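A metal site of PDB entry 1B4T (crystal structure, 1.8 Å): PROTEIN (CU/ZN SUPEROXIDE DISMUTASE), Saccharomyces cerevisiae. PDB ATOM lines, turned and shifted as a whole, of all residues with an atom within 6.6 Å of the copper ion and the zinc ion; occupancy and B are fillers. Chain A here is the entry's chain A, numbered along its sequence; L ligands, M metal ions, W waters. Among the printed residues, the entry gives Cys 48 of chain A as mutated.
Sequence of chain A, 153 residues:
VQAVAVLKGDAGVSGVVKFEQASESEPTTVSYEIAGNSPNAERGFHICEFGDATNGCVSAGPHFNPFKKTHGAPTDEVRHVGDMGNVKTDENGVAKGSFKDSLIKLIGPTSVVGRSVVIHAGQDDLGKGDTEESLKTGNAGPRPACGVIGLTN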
ATOM      1  N   GLY A  44       4.440 -21.663  27.758  1.00  0.00           N
ATOM      2  CA  GLY A  44       4.207 -20.398  27.082  1.00  0.00           C
ATOM      3  C   GLY A  44       4.511 -19.238  28.006  1.00  0.00           C
ATOM      4  O   GLY A  44       4.049 -19.232  29.132  1.00  0.00           O
ATOM      5  N   PHE A  45       5.207 -18.231  27.488  1.00  0.00           N
ATOM      6  CA  PHE A  45       5.642 -17.049  28.245  1.00  0.00           C
ATOM      7  C   PHE A  45       5.248 -15.854  27.384  1.00  0.00           C
ATOM      8  O   PHE A  45       5.874 -15.627  26.351  1.00  0.00           O
ATOM      9  CB  PHE A  45       7.156 -17.149  28.384  1.00  0.00           C
ATOM     10  CG  PHE A  45       7.780 -16.138  29.285  1.00  0.00           C
ATOM     11  CD1 PHE A  45       7.245 -15.860  30.531  1.00  0.00           C
ATOM     12  CD2 PHE A  45       8.963 -15.507  28.919  1.00  0.00           C
ATOM     13  CE1 PHE A  45       7.887 -14.967  31.412  1.00  0.00           C
ATOM     14  CE2 PHE A  45       9.616 -14.626  29.784  1.00  0.00           C
ATOM     15  CZ  PHE A  45       9.081 -14.355  31.023  1.00  0.00           C
ATOM     16  N   HIS A  46       4.225 -15.102  27.800  1.00  0.00           N
ATOM     17  CA  HIS A  46       3.742 -13.976  26.986  1.00  0.00           C
ATOM     18  C   HIS A  46       3.455 -12.694  27.733  1.00  0.00           C
ATOM     19  O   HIS A  46       3.290 -12.682  28.938  1.00  0.00           O
ATOM     20  CB  HIS A  46       2.435 -14.353  26.281  1.00  0.00           C
ATOM     21  CG  HIS A  46       2.466 -15.690  25.608  1.00  0.00           C
ATOM     22  ND1 HIS A  46       1.470 -16.634  25.780  1.00  0.00           N
ATOM     23  CD2 HIS A  46       3.360 -16.251  24.762  1.00  0.00           C
ATOM     24  CE1 HIS A  46       1.750 -17.713  25.070  1.00  0.00           C
ATOM     25  NE2 HIS A  46       2.896 -17.506  24.444  1.00  0.00           N
ATOM     26  N   ILE A  47       3.432 -11.598  26.977  1.00  0.00           N
ATOM     27  CA  ILE A  47       3.083 -10.294  27.527  1.00  0.00           C
ATOM     28  C   ILE A  47       1.687  -9.958  26.994  1.00  0.00           C
ATOM     29  O   ILE A  47       1.451 -10.012  25.780  1.00  0.00           O
ATOM     30  CB  ILE A  47       4.055  -9.192  27.110  1.00  0.00           C
ATOM     31  CG1 ILE A  47       5.433  -9.460  27.701  1.00  0.00           C
ATOM     32  CG2 ILE A  47       3.536  -7.822  27.578  1.00  0.00           C
ATOM     33  CD1 ILE A  47       6.507  -8.513  27.207  1.00  0.00           C
ATOM     34  N   CYS A  48       0.764  -9.648  27.888  1.00  0.00           N
ATOM     35  CA  CYS A  48      -0.613  -9.309  27.524  1.00  0.00           C
ATOM     36  C   CYS A  48      -0.875  -7.805  27.514  1.00  0.00           C
ATOM     37  O   CYS A  48      -0.148  -7.018  28.125  1.00  0.00           O
ATOM     38  CB  CYS A  48      -1.614 -10.074  28.409  1.00  0.00           C
ATOM     39  SG  CYS A  48      -1.616 -11.850  28.114  1.00  0.00           S
ATOM     40  N   HIS A  63      -2.751 -11.240  24.004  1.00  0.00           N
ATOM     41  CA  HIS A  63      -1.348 -10.898  23.846  1.00  0.00           C
ATOM     42  C   HIS A  63      -1.244  -9.478  23.288  1.00  0.00           C
ATOM     43  O   HIS A  63      -2.078  -9.076  22.471  1.00  0.00           O
ATOM     44  CB  HIS A  63      -0.705 -11.854  22.877  1.00  0.00           C
ATOM     45  CG  HIS A  63      -0.669 -13.257  23.361  1.00  0.00           C
ATOM     46  ND1 HIS A  63      -0.383 -14.318  22.534  1.00  0.00           N
ATOM     47  CD2 HIS A  63      -0.818 -13.783  24.609  1.00  0.00           C
ATOM     48  CE1 HIS A  63      -0.353 -15.433  23.240  1.00  0.00           C
ATOM     49  NE2 HIS A  63      -0.608 -15.131  24.501  1.00  0.00           N
ATOM     50  N   PHE A  64      -0.234  -8.722  23.730  1.00  0.00           N
ATOM     51  CA  PHE A  64      -0.037  -7.367  23.244  1.00  0.00           C
ATOM     52  C   PHE A  64       0.229  -7.486  21.731  1.00  0.00           C
ATOM     53  O   PHE A  64       1.158  -8.168  21.307  1.00  0.00           O
ATOM     54  CB  PHE A  64       1.103  -6.697  23.982  1.00  0.00           C
ATOM     55  CG  PHE A  64       1.224  -5.233  23.707  1.00  0.00           C
ATOM     56  CD1 PHE A  64       0.088  -4.438  23.560  1.00  0.00           C
ATOM     57  CD2 PHE A  64       2.483  -4.637  23.595  1.00  0.00           C
ATOM     58  CE1 PHE A  64       0.203  -3.085  23.311  1.00  0.00           C
ATOM     59  CE2 PHE A  64       2.603  -3.269  23.344  1.00  0.00           C
ATOM     60  CZ  PHE A  64       1.452  -2.492  23.200  1.00  0.00           C
ATOM     61  N   THR A  70      -0.788 -12.171  13.628  1.00  0.00           N
ATOM     62  CA  THR A  70      -1.159 -13.429  14.285  1.00  0.00           C
ATOM     63  C   THR A  70      -0.059 -13.916  15.225  1.00  0.00           C
ATOM     64  O   THR A  70       1.047 -13.385  15.219  1.00  0.00           O
ATOM     65  CB  THR A  70      -1.500 -14.554  13.266  1.00  0.00           C
ATOM     66  OG1 THR A  70      -0.467 -14.636  12.281  1.00  0.00           O
ATOM     67  CG2 THR A  70      -2.832 -14.280  12.588  1.00  0.00           C
ATOM     68  N   HIS A  71      -0.389 -14.917  16.038  1.00  0.00           N
ATOM     69  CA  HIS A  71       0.545 -15.477  16.994  1.00  0.00           C
ATOM     70  C   HIS A  71       1.657 -16.275  16.305  1.00  0.00           C
ATOM     71  O   HIS A  71       1.393 -17.117  15.437  1.00  0.00           O
ATOM     72  CB  HIS A  71      -0.198 -16.379  17.997  1.00  0.00           C
ATOM     73  CG  HIS A  71       0.682 -16.934  19.070  1.00  0.00           C
ATOM     74  ND1 HIS A  71       0.967 -16.244  20.233  1.00  0.00           N
ATOM     75  CD2 HIS A  71       1.420 -18.069  19.123  1.00  0.00           C
ATOM     76  CE1 HIS A  71       1.845 -16.919  20.944  1.00  0.00           C
ATOM     77  NE2 HIS A  71       2.133 -18.026  20.292  1.00  0.00           N
ATOM     78  N   GLY A  72       2.890 -16.037  16.733  1.00  0.00           N
ATOM     79  CA  GLY A  72       4.024 -16.728  16.152  1.00  0.00           C
ATOM     80  C   GLY A  72       5.112 -16.919  17.178  1.00  0.00           C
ATOM     81  O   GLY A  72       4.891 -16.746  18.373  1.00  0.00           O
ATOM     82  N   ARG A  79       4.250 -12.063  14.206  1.00  0.00           N
ATOM     83  CA  ARG A  79       4.065 -12.484  15.586  1.00  0.00           C
ATOM     84  C   ARG A  79       3.499 -11.292  16.341  1.00  0.00           C
ATOM     85  O   ARG A  79       3.538 -10.154  15.875  1.00  0.00           O
ATOM     86  CB  ARG A  79       5.407 -12.864  16.216  1.00  0.00           C
ATOM     87  CG  ARG A  79       6.461 -11.760  16.144  1.00  0.00           C
ATOM     88  CD  ARG A  79       7.656 -11.994  17.052  1.00  0.00           C
ATOM     89  NE  ARG A  79       7.550 -11.301  18.333  1.00  0.00           N
ATOM     90  CZ  ARG A  79       8.582 -10.895  19.069  1.00  0.00           C
ATOM     91  NH1 ARG A  79       9.826 -11.104  18.655  1.00  0.00           N
ATOM     92  NH2 ARG A  79       8.388 -10.238  20.208  1.00  0.00           N
ATOM     93  N   HIS A  80       2.974 -11.559  17.523  1.00  0.00           N
ATOM     94  CA  HIS A  80       2.467 -10.507  18.394  1.00  0.00           C
ATOM     95  C   HIS A  80       3.708  -9.934  19.083  1.00  0.00           C
ATOM     96  O   HIS A  80       4.711 -10.611  19.198  1.00  0.00           O
ATOM     97  CB  HIS A  80       1.557 -11.096  19.466  1.00  0.00           C
ATOM     98  CG  HIS A  80       0.320 -11.735  18.930  1.00  0.00           C
ATOM     99  ND1 HIS A  80      -0.274 -12.826  19.540  1.00  0.00           N
ATOM    100  CD2 HIS A  80      -0.481 -11.409  17.894  1.00  0.00           C
ATOM    101  CE1 HIS A  80      -1.391 -13.124  18.901  1.00  0.00           C
ATOM    102  NE2 HIS A  80      -1.537 -12.278  17.901  1.00  0.00           N
ATOM    103  N   VAL A  81       3.621  -8.705  19.575  1.00  0.00           N
ATOM    104  CA  VAL A  81       4.761  -8.101  20.279  1.00  0.00           C
ATOM    105  C   VAL A  81       5.048  -8.884  21.569  1.00  0.00           C
ATOM    106  O   VAL A  81       6.198  -9.137  21.911  1.00  0.00           O
ATOM    107  CB  VAL A  81       4.513  -6.591  20.590  1.00  0.00           C
ATOM    108  CG1 VAL A  81       5.506  -6.082  21.616  1.00  0.00           C
ATOM    109  CG2 VAL A  81       4.595  -5.767  19.308  1.00  0.00           C
ATOM    110  N   GLY A  82       3.991  -9.302  22.258  1.00  0.00           N
ATOM    111  CA  GLY A  82       4.143 -10.055  23.491  1.00  0.00           C
ATOM    112  C   GLY A  82       4.474 -11.531  23.338  1.00  0.00           C
ATOM    113  O   GLY A  82       4.381 -12.294  24.304  1.00  0.00           O
ATOM    114  N   ASP A  83       4.857 -11.953  22.137  1.00  0.00           N
ATOM    115  CA  ASP A  83       5.187 -13.340  21.881  1.00  0.00           C
ATOM    116  C   ASP A  83       6.634 -13.622  22.195  1.00  0.00           C
ATOM    117  O   ASP A  83       7.525 -13.371  21.389  1.00  0.00           O
ATOM    118  CB  ASP A  83       4.893 -13.721  20.436  1.00  0.00           C
ATOM    119  CG  ASP A  83       3.411 -13.888  20.185  1.00  0.00           C
ATOM    120  OD1 ASP A  83       2.633 -13.942  21.160  1.00  0.00           O
ATOM    121  OD2 ASP A  83       3.023 -13.976  19.006  1.00  0.00           O
ATOM    122  N   VAL A 118       2.592 -12.993  31.493  1.00  0.00           N
ATOM    123  CA  VAL A 118       1.856 -14.199  31.837  1.00  0.00           C
ATOM    124  C   VAL A 118       2.678 -15.453  31.536  1.00  0.00           C
ATOM    125  O   VAL A 118       3.374 -15.522  30.507  1.00  0.00           O
ATOM    126  CB  VAL A 118       0.497 -14.245  31.052  1.00  0.00           C
ATOM    127  CG1 VAL A 118      -0.121 -15.634  31.080  1.00  0.00           C
ATOM    128  CG2 VAL A 118      -0.490 -13.244  31.634  1.00  0.00           C
ATOM    129  N   HIS A 120       2.224 -19.596  31.128  1.00  0.00           N
ATOM    130  CA  HIS A 120       1.175 -20.570  30.843  1.00  0.00           C
ATOM    131  C   HIS A 120       1.319 -21.924  31.472  1.00  0.00           C
ATOM    132  O   HIS A 120       2.416 -22.294  31.870  1.00  0.00           O
ATOM    133  CB  HIS A 120       1.021 -20.759  29.347  1.00  0.00           C
ATOM    134  CG  HIS A 120       0.313 -19.629  28.693  1.00  0.00           C
ATOM    135  ND1 HIS A 120      -1.063 -19.501  28.723  1.00  0.00           N
ATOM    136  CD2 HIS A 120       0.774 -18.522  28.069  1.00  0.00           C
ATOM    137  CE1 HIS A 120      -1.408 -18.370  28.157  1.00  0.00           C
ATOM    138  NE2 HIS A 120      -0.311 -17.755  27.756  1.00  0.00           N
ATOM    139  N   ASP A 124       3.311 -23.476  24.183  1.00  0.00           N
ATOM    140  CA  ASP A 124       2.911 -22.616  23.076  1.00  0.00           C
ATOM    141  C   ASP A 124       3.285 -23.354  21.765  1.00  0.00           C
ATOM    142  O   ASP A 124       4.447 -23.675  21.540  1.00  0.00           O
ATOM    143  CB  ASP A 124       3.710 -21.305  23.242  1.00  0.00           C
ATOM    144  CG  ASP A 124       3.371 -20.232  22.210  1.00  0.00           C
ATOM    145  OD1 ASP A 124       2.654 -20.484  21.236  1.00  0.00           O
ATOM    146  OD2 ASP A 124       3.866 -19.106  22.391  1.00  0.00           O
ATOM    147  N   LEU A 135      -3.482 -19.441  16.223  1.00  0.00           N
ATOM    148  CA  LEU A 135      -3.127 -18.115  15.696  1.00  0.00           C
ATOM    149  C   LEU A 135      -3.385 -16.967  16.637  1.00  0.00           C
ATOM    150  O   LEU A 135      -3.166 -15.798  16.282  1.00  0.00           O
ATOM    151  CB  LEU A 135      -3.849 -17.843  14.369  1.00  0.00           C
ATOM    152  CG  LEU A 135      -3.429 -18.680  13.161  1.00  0.00           C
ATOM    153  CD1 LEU A 135      -4.339 -18.301  12.005  1.00  0.00           C
ATOM    154  CD2 LEU A 135      -1.947 -18.475  12.822  1.00  0.00           C
ATOM    155  N   LYS A 136      -3.902 -17.262  17.819  1.00  0.00           N
ATOM    156  CA  LYS A 136      -4.135 -16.225  18.787  1.00  0.00           C
ATOM    157  C   LYS A 136      -3.391 -16.439  20.088  1.00  0.00           C
ATOM    158  O   LYS A 136      -2.741 -15.524  20.579  1.00  0.00           O
ATOM    159  CB  LYS A 136      -5.630 -16.022  19.029  1.00  0.00           C
ATOM    160  CG  LYS A 136      -6.473 -17.252  19.033  1.00  0.00           C
ATOM    161  CD  LYS A 136      -7.785 -16.948  19.743  1.00  0.00           C
ATOM    162  CE  LYS A 136      -8.454 -15.656  19.256  1.00  0.00           C
ATOM    163  NZ  LYS A 136      -8.793 -15.690  17.787  1.00  0.00           N
ATOM    164  N   THR A 137      -3.417 -17.669  20.605  1.00  0.00           N
ATOM    165  CA  THR A 137      -2.770 -17.974  21.875  1.00  0.00           C
ATOM    166  C   THR A 137      -1.653 -19.020  21.775  1.00  0.00           C
ATOM    167  O   THR A 137      -0.858 -19.200  22.707  1.00  0.00           O
ATOM    168  CB  THR A 137      -3.799 -18.478  22.936  1.00  0.00           C
ATOM    169  OG1 THR A 137      -4.337 -19.751  22.530  1.00  0.00           O
ATOM    170  CG2 THR A 137      -4.948 -17.514  23.087  1.00  0.00           C
ATOM    171  N   GLY A 138      -1.547 -19.671  20.622  1.00  0.00           N
ATOM    172  CA  GLY A 138      -0.553 -20.698  20.506  1.00  0.00           C
ATOM    173  C   GLY A 138      -1.042 -21.924  21.261  1.00  0.00           C
ATOM    174  O   GLY A 138      -0.288 -22.881  21.435  1.00  0.00           O
ATOM    175  N   ALA A 140      -1.648 -22.364  24.364  1.00  0.00           N
ATOM    176  CA  ALA A 140      -0.853 -22.570  25.548  1.00  0.00           C
ATOM    177  C   ALA A 140      -1.599 -22.870  26.855  1.00  0.00           C
ATOM    178  O   ALA A 140      -0.984 -23.012  27.903  1.00  0.00           O
ATOM    179  CB  ALA A 140       0.107 -21.392  25.705  1.00  0.00           C
ATOM    180  N   GLY A 141      -2.926 -22.903  26.796  1.00  0.00           N
ATOM    181  CA  GLY A 141      -3.693 -23.243  27.986  1.00  0.00           C
ATOM    182  C   GLY A 141      -3.871 -22.163  29.030  1.00  0.00           C
ATOM    183  O   GLY A 141      -3.689 -20.975  28.738  1.00  0.00           O
ATOM    184  N   ARG A 143      -3.505 -19.698  32.563  1.00  0.00           N
ATOM    185  CA  ARG A 143      -2.502 -18.761  33.008  1.00  0.00           C
ATOM    186  C   ARG A 143      -2.349 -18.903  34.522  1.00  0.00           C
ATOM    187  O   ARG A 143      -3.043 -18.213  35.272  1.00  0.00           O
ATOM    188  CB  ARG A 143      -2.962 -17.328  32.725  1.00  0.00           C
ATOM    189  CG  ARG A 143      -3.381 -17.070  31.310  1.00  0.00           C
ATOM    190  CD  ARG A 143      -4.015 -15.708  31.181  1.00  0.00           C
ATOM    191  NE  ARG A 143      -4.525 -15.496  29.833  1.00  0.00           N
ATOM    192  CZ  ARG A 143      -4.853 -14.318  29.321  1.00  0.00           C
ATOM    193  NH1 ARG A 143      -4.736 -13.220  30.048  1.00  0.00           N
ATOM    194  NH2 ARG A 143      -5.265 -14.243  28.075  1.00  0.00           N
HETATM  195 CL1  LIG L   1      -2.164 -15.373  27.064  1.00  0.00          CL
HETATM  196 CU    CU M   1      -0.446 -16.298  26.219  1.00  0.00          CU
HETATM  197 ZN    ZN M   2       0.643 -14.231  20.827  1.00  0.00          ZN
HETATM  198  O   HOH W   1      -1.868 -18.118  24.862  1.00  0.00           O
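The copper ion is bound by a ring nitrogen (ND1) of His 46 (2.0 Å), a ring nitrogen (NE2) of His 63 (2.1 Å), a ring nitrogen (NE2) of His 120 (2.1 Å) and a chlorine (CL1) of the ligand (2.1 Å).
The copper ion has four donor atoms within binding distance.
Slightly farther from the copper ion lies water W1 (2.7 Å).
The nearest printed residue that does not touch the copper ion is Thr 137 (4.6 Å).
A ring nitrogen (ND1) of His 120 is in hydrogen-bond range of the backbone carbonyl oxygen of Gly 141 (3.0 Å).
The guanidinium group (NH2) of Arg 79 sits at hydrogen-bond distance from the backbone carbonyl oxygen (O) of Asp 83 (3.5 Å).
The backbone carbonyl oxygen (O) of His 46 lies within hydrogen-bond range of the backbone NH (N) of Val 118 (2.7 Å).
The backbone NH (N) of His 71 sits at hydrogen-bond distance from the backbone carbonyl oxygen (O) of Leu 135 (2.9 Å).
The backbone NH (N) of His 120 lies within hydrogen-bond range of the backbone carbonyl oxygen (O) of Gly 44, at 2.7 Å.
The side-chain carboxylate of Asp 83 is in hydrogen-bond range of the backbone NH of Gly 72 (3.1 Å).
A ring nitrogen (NE2) of His 71 sits at hydrogen-bond distance from the side-chain carboxylate (OD1) of Asp 124 (2.7 Å).
A ring nitrogen (ND1) of His 63 sits close to the backbone carbonyl oxygen (O) of Lys 136.
The zinc ion is bound by a ring nitrogen (ND1) of His 63 (2.0 Å), the side-chain carboxylate (OD1) of Asp 83 (2.0 Å), a ring nitrogen (ND1) of His 80 (2.1 Å) and a ring nitrogen (ND1) of His 71 (2.1 Å).
O of Lys 136 touches the zinc ion, at 3.6 Å.
Five residues have an atom within 4 Å of the zinc ion: His 63, His 71, His 80, Asp 83 and Lys 136.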
